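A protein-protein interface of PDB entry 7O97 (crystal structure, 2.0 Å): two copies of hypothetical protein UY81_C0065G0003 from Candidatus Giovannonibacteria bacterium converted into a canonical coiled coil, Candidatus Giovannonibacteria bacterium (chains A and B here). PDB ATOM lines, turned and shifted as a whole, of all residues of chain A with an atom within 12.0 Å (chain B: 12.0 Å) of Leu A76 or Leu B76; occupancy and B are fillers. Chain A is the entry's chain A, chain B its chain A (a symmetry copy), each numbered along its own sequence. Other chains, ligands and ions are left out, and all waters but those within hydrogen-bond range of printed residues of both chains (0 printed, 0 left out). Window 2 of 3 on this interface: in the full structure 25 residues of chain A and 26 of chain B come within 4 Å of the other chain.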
ATOM      1  N   ASP A  67      -1.282 -16.729  13.271  1.00  0.00           N
ATOM      2  CA  ASP A  67       0.055 -16.361  12.747  1.00  0.00           C
ATOM      3  C   ASP A  67       0.026 -14.963  12.110  1.00  0.00           C
ATOM      4  O   ASP A  67       0.936 -14.163  12.347  1.00  0.00           O
ATOM      5  CB  ASP A  67       0.584 -17.405  11.704  1.00  0.00           C
ATOM      6  CG  ASP A  67       1.010 -18.756  12.345  1.00  0.00           C
ATOM      7  OD1 ASP A  67       1.358 -18.785  13.543  1.00  0.00           O
ATOM      8  OD2 ASP A  67       1.019 -19.798  11.641  1.00  0.00           O
ATOM      9  N   ARG A  68      -1.016 -14.655  11.331  1.00  0.00           N
ATOM     10  CA  ARG A  68      -1.127 -13.338  10.666  1.00  0.00           C
ATOM     11  C   ARG A  68      -1.370 -12.184  11.629  1.00  0.00           C
ATOM     12  O   ARG A  68      -0.795 -11.099  11.506  1.00  0.00           O
ATOM     13  CB  ARG A  68      -2.196 -13.383   9.590  1.00  0.00           C
ATOM     14  CG  ARG A  68      -1.789 -14.252   8.408  1.00  0.00           C
ATOM     15  CD  ARG A  68      -2.930 -14.434   7.421  1.00  0.00           C
ATOM     16  NE  ARG A  68      -3.383 -13.159   6.841  1.00  0.00           N
ATOM     17  CZ  ARG A  68      -4.466 -13.015   6.067  1.00  0.00           C
ATOM     18  NH1 ARG A  68      -5.219 -14.067   5.744  1.00  0.00           N
ATOM     19  NH2 ARG A  68      -4.816 -11.814   5.616  1.00  0.00           N
ATOM     20  N   ILE A  69      -2.178 -12.425  12.636  1.00  0.00           N
ATOM     21  CA  ILE A  69      -2.308 -11.444  13.692  1.00  0.00           C
ATOM     22  C   ILE A  69      -0.960 -11.260  14.393  1.00  0.00           C
ATOM     23  O   ILE A  69      -0.533 -10.145  14.558  1.00  0.00           O
ATOM     24  CB  ILE A  69      -3.440 -11.804  14.666  1.00  0.00           C
ATOM     25  CG1 ILE A  69      -4.782 -11.635  13.950  1.00  0.00           C
ATOM     26  CG2 ILE A  69      -3.427 -10.902  15.894  1.00  0.00           C
ATOM     27  CD1 ILE A  69      -5.850 -12.579  14.452  1.00  0.00           C
ATOM     28  N   GLY A  70      -0.286 -12.333  14.794  1.00  0.00           N
ATOM     29  CA  GLY A  70       1.064 -12.206  15.334  1.00  0.00           C
ATOM     30  C   GLY A  70       2.013 -11.310  14.549  1.00  0.00           C
ATOM     31  O   GLY A  70       2.691 -10.452  15.132  1.00  0.00           O
ATOM     32  N   ARG A  71       2.065 -11.504  13.233  1.00  0.00           N
ATOM     33  CA  ARG A  71       2.966 -10.747  12.358  1.00  0.00           C
ATOM     34  C   ARG A  71       2.671  -9.265  12.478  1.00  0.00           C
ATOM     35  O   ARG A  71       3.588  -8.447  12.555  1.00  0.00           O
ATOM     36  CB  ARG A  71       2.816 -11.159  10.879  1.00  0.00           C
ATOM     37  CG  ARG A  71       3.955 -11.952  10.249  1.00  0.00           C
ATOM     38  CD  ARG A  71       3.573 -12.338   8.822  1.00  0.00           C
ATOM     39  NE  ARG A  71       2.604 -13.454   8.785  1.00  0.00           N
ATOM     40  CZ  ARG A  71       2.087 -13.999   7.680  1.00  0.00           C
ATOM     41  NH1 ARG A  71       2.414 -13.533   6.480  1.00  0.00           N
ATOM     42  NH2 ARG A  71       1.234 -15.021   7.766  1.00  0.00           N
ATOM     43  N   VAL A  72       1.383  -8.935  12.493  1.00  0.00           N
ATOM     44  CA  VAL A  72       0.946  -7.548  12.528  1.00  0.00           C
ATOM     45  C   VAL A  72       1.093  -6.892  13.905  1.00  0.00           C
ATOM     46  O   VAL A  72       1.588  -5.770  13.978  1.00  0.00           O
ATOM     47  CB  VAL A  72      -0.499  -7.423  12.026  1.00  0.00           C
ATOM     48  CG1 VAL A  72      -0.998  -6.006  12.198  1.00  0.00           C
ATOM     49  CG2 VAL A  72      -0.573  -7.815  10.562  1.00  0.00           C
ATOM     50  N   GLU A  73       0.650  -7.570  14.975  1.00  0.00           N
ATOM     51  CA  GLU A  73       0.803  -7.070  16.357  1.00  0.00           C
ATOM     52  C   GLU A  73       2.265  -6.705  16.612  1.00  0.00           C
ATOM     53  O   GLU A  73       2.546  -5.654  17.197  1.00  0.00           O
ATOM     54  CB  GLU A  73       0.330  -8.090  17.430  1.00  0.00           C
ATOM     55  CG  GLU A  73      -1.180  -8.437  17.416  1.00  0.00           C
ATOM     56  CD  GLU A  73      -1.890  -8.690  18.794  1.00  0.00           C
ATOM     57  OE1 GLU A  73      -2.114  -9.887  19.135  1.00  0.00           O
ATOM     58  OE2 GLU A  73      -2.298  -7.716  19.521  1.00  0.00           O
ATOM     59  N   SER A  74       3.188  -7.556  16.145  1.00  0.00           N
ATOM     60  CA  SER A  74       4.634  -7.325  16.347  1.00  0.00           C
ATOM     61  C   SER A  74       5.171  -6.220  15.427  1.00  0.00           C
ATOM     62  O   SER A  74       5.963  -5.393  15.860  1.00  0.00           O
ATOM     63  CB  SER A  74       5.450  -8.623  16.157  1.00  0.00           C
ATOM     64  OG  SER A  74       5.862  -8.779  14.805  1.00  0.00           O
ATOM     65  N   LYS A  75       4.717  -6.191  14.171  1.00  0.00           N
ATOM     66  CA  LYS A  75       5.248  -5.230  13.200  1.00  0.00           C
ATOM     67  C   LYS A  75       4.790  -3.841  13.562  1.00  0.00           C
ATOM     68  O   LYS A  75       5.603  -2.932  13.657  1.00  0.00           O
ATOM     69  CB  LYS A  75       4.879  -5.607  11.765  1.00  0.00           C
ATOM     70  CG  LYS A  75       5.875  -6.648  11.218  1.00  0.00           C
ATOM     71  CD  LYS A  75       5.381  -7.509  10.049  1.00  0.00           C
ATOM     72  CE  LYS A  75       5.457  -6.779   8.712  1.00  0.00           C
ATOM     73  NZ  LYS A  75       4.445  -5.681   8.602  1.00  0.00           N
ATOM     74  N   LEU A  76       3.496  -3.698  13.820  1.00  0.00           N
ATOM     75  CA  LEU A  76       2.947  -2.494  14.460  1.00  0.00           C
ATOM     76  C   LEU A  76       3.878  -1.907  15.553  1.00  0.00           C
ATOM     77  O   LEU A  76       3.946  -0.693  15.705  1.00  0.00           O
ATOM     78  CB  LEU A  76       1.567  -2.803  15.050  1.00  0.00           C
ATOM     79  CG  LEU A  76       0.627  -1.657  15.439  1.00  0.00           C
ATOM     80  CD1 LEU A  76      -0.220  -1.212  14.253  1.00  0.00           C
ATOM     81  CD2 LEU A  76      -0.267  -2.062  16.607  1.00  0.00           C
ATOM     82  N   ASP A  77       4.593  -2.748  16.303  1.00  0.00           N
ATOM     83  CA  ASP A  77       5.575  -2.265  17.294  1.00  0.00           C
ATOM     84  C   ASP A  77       6.994  -2.233  16.736  1.00  0.00           C
ATOM     85  O   ASP A  77       7.546  -1.172  16.514  1.00  0.00           O
ATOM     86  CB  ASP A  77       5.554  -3.151  18.536  1.00  0.00           C
ATOM     87  CG  ASP A  77       4.148  -3.504  18.964  1.00  0.00           C
ATOM     88  OD1 ASP A  77       3.234  -2.664  18.784  1.00  0.00           O
ATOM     89  OD2 ASP A  77       3.963  -4.634  19.461  1.00  0.00           O
ATOM     90  N   ASP B  67     -10.983 -10.986   6.188  1.00  0.00           N
ATOM     91  CA  ASP B  67     -11.172  -9.654   5.566  1.00  0.00           C
ATOM     92  C   ASP B  67     -10.601  -8.545   6.464  1.00  0.00           C
ATOM     93  O   ASP B  67      -9.925  -7.640   5.966  1.00  0.00           O
ATOM     94  CB  ASP B  67     -12.681  -9.359   5.258  1.00  0.00           C
ATOM     95  CG  ASP B  67     -13.242 -10.192   4.070  1.00  0.00           C
ATOM     96  OD1 ASP B  67     -12.460 -10.619   3.196  1.00  0.00           O
ATOM     97  OD2 ASP B  67     -14.479 -10.404   3.996  1.00  0.00           O
ATOM     98  N   ARG B  68     -10.844  -8.620   7.777  1.00  0.00           N
ATOM     99  CA  ARG B  68     -10.347  -7.594   8.719  1.00  0.00           C
ATOM    100  C   ARG B  68      -8.834  -7.604   8.892  1.00  0.00           C
ATOM    101  O   ARG B  68      -8.177  -6.561   8.944  1.00  0.00           O
ATOM    102  CB  ARG B  68     -11.046  -7.731  10.059  1.00  0.00           C
ATOM    103  CG  ARG B  68     -12.516  -7.341   9.984  1.00  0.00           C
ATOM    104  CD  ARG B  68     -13.249  -7.646  11.280  1.00  0.00           C
ATOM    105  NE  ARG B  68     -12.698  -6.907  12.427  1.00  0.00           N
ATOM    106  CZ  ARG B  68     -13.053  -7.103  13.704  1.00  0.00           C
ATOM    107  NH1 ARG B  68     -13.981  -8.006  14.022  1.00  0.00           N
ATOM    108  NH2 ARG B  68     -12.474  -6.408  14.677  1.00  0.00           N
ATOM    109  N   ILE B  69      -8.257  -8.784   8.918  1.00  0.00           N
ATOM    110  CA  ILE B  69      -6.811  -8.868   8.887  1.00  0.00           C
ATOM    111  C   ILE B  69      -6.290  -8.279   7.573  1.00  0.00           C
ATOM    112  O   ILE B  69      -5.402  -7.464   7.609  1.00  0.00           O
ATOM    113  CB  ILE B  69      -6.321 -10.302   9.132  1.00  0.00           C
ATOM    114  CG1 ILE B  69      -6.600 -10.680  10.588  1.00  0.00           C
ATOM    115  CG2 ILE B  69      -4.825 -10.431   8.873  1.00  0.00           C
ATOM    116  CD1 ILE B  69      -6.860 -12.156  10.783  1.00  0.00           C
ATOM    117  N   GLY B  70      -6.833  -8.671   6.426  1.00  0.00           N
ATOM    118  CA  GLY B  70      -6.463  -8.028   5.168  1.00  0.00           C
ATOM    119  C   GLY B  70      -6.425  -6.505   5.186  1.00  0.00           C
ATOM    120  O   GLY B  70      -5.452  -5.897   4.718  1.00  0.00           O
ATOM    121  N   ARG B  71      -7.475  -5.888   5.722  1.00  0.00           N
ATOM    122  CA  ARG B  71      -7.597  -4.427   5.765  1.00  0.00           C
ATOM    123  C   ARG B  71      -6.426  -3.839   6.526  1.00  0.00           C
ATOM    124  O   ARG B  71      -5.846  -2.836   6.109  1.00  0.00           O
ATOM    125  CB  ARG B  71      -8.903  -3.975   6.449  1.00  0.00           C
ATOM    126  CG  ARG B  71      -9.989  -3.370   5.567  1.00  0.00           C
ATOM    127  CD  ARG B  71     -11.224  -3.077   6.414  1.00  0.00           C
ATOM    128  NE  ARG B  71     -11.987  -4.303   6.732  1.00  0.00           N
ATOM    129  CZ  ARG B  71     -13.106  -4.357   7.461  1.00  0.00           C
ATOM    130  NH1 ARG B  71     -13.621  -3.253   7.991  1.00  0.00           N
ATOM    131  NH2 ARG B  71     -13.724  -5.521   7.666  1.00  0.00           N
ATOM    132  N   VAL B  72      -6.087  -4.476   7.642  1.00  0.00           N
ATOM    133  CA  VAL B  72      -5.033  -3.987   8.518  1.00  0.00           C
ATOM    134  C   VAL B  72      -3.620  -4.249   7.984  1.00  0.00           C
ATOM    135  O   VAL B  72      -2.796  -3.339   8.016  1.00  0.00           O
ATOM    136  CB  VAL B  72      -5.189  -4.567   9.930  1.00  0.00           C
ATOM    137  CG1 VAL B  72      -4.015  -4.172  10.797  1.00  0.00           C
ATOM    138  CG2 VAL B  72      -6.476  -4.064  10.557  1.00  0.00           C
ATOM    139  N   GLU B  73      -3.341  -5.478   7.523  1.00  0.00           N
ATOM    140  CA  GLU B  73      -2.038  -5.826   6.919  1.00  0.00           C
ATOM    141  C   GLU B  73      -1.700  -4.829   5.813  1.00  0.00           C
ATOM    142  O   GLU B  73      -0.560  -4.364   5.727  1.00  0.00           O
ATOM    143  CB  GLU B  73      -2.000  -7.270   6.343  1.00  0.00           C
ATOM    144  CG  GLU B  73      -2.154  -8.415   7.374  1.00  0.00           C
ATOM    145  CD  GLU B  73      -1.337  -9.735   7.136  1.00  0.00           C
ATOM    146  OE1 GLU B  73      -1.949 -10.734   6.659  1.00  0.00           O
ATOM    147  OE2 GLU B  73      -0.105  -9.826   7.479  1.00  0.00           O
ATOM    148  N   SER B  74      -2.700  -4.478   4.992  1.00  0.00           N
ATOM    149  CA  SER B  74      -2.495  -3.537   3.871  1.00  0.00           C
ATOM    150  C   SER B  74      -2.370  -2.087   4.356  1.00  0.00           C
ATOM    151  O   SER B  74      -1.530  -1.345   3.862  1.00  0.00           O
ATOM    152  CB  SER B  74      -3.618  -3.654   2.816  1.00  0.00           C
ATOM    153  OG  SER B  74      -4.692  -2.768   3.108  1.00  0.00           O
ATOM    154  N   LYS B  75      -3.184  -1.695   5.341  1.00  0.00           N
ATOM    155  CA  LYS B  75      -3.198  -0.303   5.798  1.00  0.00           C
ATOM    156  C   LYS B  75      -1.915   0.001   6.528  1.00  0.00           C
ATOM    157  O   LYS B  75      -1.251   0.981   6.219  1.00  0.00           O
ATOM    158  CB  LYS B  75      -4.434   0.007   6.644  1.00  0.00           C
ATOM    159  CG  LYS B  75      -5.630   0.337   5.731  1.00  0.00           C
ATOM    160  CD  LYS B  75      -7.023   0.153   6.347  1.00  0.00           C
ATOM    161  CE  LYS B  75      -7.424   1.319   7.244  1.00  0.00           C
ATOM    162  NZ  LYS B  75      -6.638   1.357   8.518  1.00  0.00           N
ATOM    163  N   LEU B  76      -1.544  -0.874   7.454  1.00  0.00           N
ATOM    164  CA  LEU B  76      -0.197  -0.878   8.041  1.00  0.00           C
ATOM    165  C   LEU B  76       0.915  -0.532   7.018  1.00  0.00           C
ATOM    166  O   LEU B  76       1.890   0.118   7.376  1.00  0.00           O
ATOM    167  CB  LEU B  76       0.083  -2.239   8.687  1.00  0.00           C
ATOM    168  CG  LEU B  76       1.243  -2.391   9.678  1.00  0.00           C
ATOM    169  CD1 LEU B  76       0.804  -2.050  11.098  1.00  0.00           C
ATOM    170  CD2 LEU B  76       1.818  -3.803   9.625  1.00  0.00           C
ATOM    171  N   ASP B  77       0.777  -0.950   5.757  1.00  0.00           N
ATOM    172  CA  ASP B  77       1.739  -0.577   4.702  1.00  0.00           C
ATOM    173  C   ASP B  77       1.280   0.634   3.900  1.00  0.00           C
ATOM    174  O   ASP B  77       1.853   1.702   4.009  1.00  0.00           O
ATOM    175  CB  ASP B  77       1.959  -1.747   3.748  1.00  0.00           C
ATOM    176  CG  ASP B  77       2.097  -3.063   4.477  1.00  0.00           C
ATOM    177  OD1 ASP B  77       2.643  -3.072   5.607  1.00  0.00           O
ATOM    178  OD2 ASP B  77       1.639  -4.082   3.920  1.00  0.00           O
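Of the printed residues of chain B, Arg A68 touches Ile B69, Gly B70 and Glu B73. Printed residues of chain B within 4 Å of Ile A69: Ile B69. Of chain B, only Val B72 (3.8 Å) and Glu B73 (3.6 Å) come within 4 Å of Val A72. Lys A75 touches one residue of chain B. Leu A76 touches just one residue of chain B: Leu B76. No residue of chain B comes within 4 Å of Asp A77. Of the printed residues of chain A, Ile B69 touches Arg A68 and Ile A69. Of the printed residues of chain A, Gly B70 touches Arg A68 (3.8 Å). Val B72 touches just one residue of chain A: Val A72 (3.8 Å). No residue of chain A comes within 4 Å of Ser B74. No residue of chain A comes within 4 Å of Lys B75. Of chain A, only Lys A75 and Leu A76 come within 4 Å of Leu B76. No residue of chain A comes within 4 Å of Asp B77. The nearest residue of chain B that does not touch Leu A76 is Val B72 (5.9 Å).
Printed residues of chain A that touch a printed residue of chain B: Arg A68, Ile A69, Val A72, Lys A75 and Leu A76. Of the 11 printed residues of chain B, 5 touch a printed residue of chain A. Hydrophobic or aromatic side chains of chain B within 4 Å of the printed part of chain A: Ile B69, Val B72 and Leu B76. Among the printed residues, Asp or Glu carboxylates within 4 Å of a Lys or Arg side-chain nitrogen of the other chain: Arg A68 with Glu B73 (2.8 Å).
NE of Arg A68 lies within salt-bridge range of OE1 of Glu B73 (2.8 Å).
Arg A68 touches Glu B73, but with the chains exchanged Glu A73 does not touch Arg B68 (10.7 Å). Ile A69 touches its own counterpart, Ile B69. Val B72 touches its own counterpart, Val A72. Val A72 touches Glu B73, but with the chains exchanged Glu A73 does not touch Val B72 (7.1 Å). Positions printed for both chains: 67, 68, 69, 70, 71, 72, 73, 74, 75, 76 and 77. Of the 8 pairs that touch across the chains among the printed residues, 3 have their exchanged pair printed and touching as well.
CG2 of Ile B69 touches NH2 of Arg A68, 3.5 Å away. NH2 of Arg A68 touches N of Gly B70, 3.8 Å away. CD1 of Ile B69 touches CG1 of Ile A69, 3.8 Å away. Val A72 touches Val B72 (CG1 to CG1, 3.8 Å). CG2 of Val A72 touches CG of Glu B73, at 3.6 Å. Leu B76 touches Lys A75 (CD2 to NZ, 3.4 Å). CD1 of Leu B76 touches CD1 of Leu A76 (3.4 Å).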
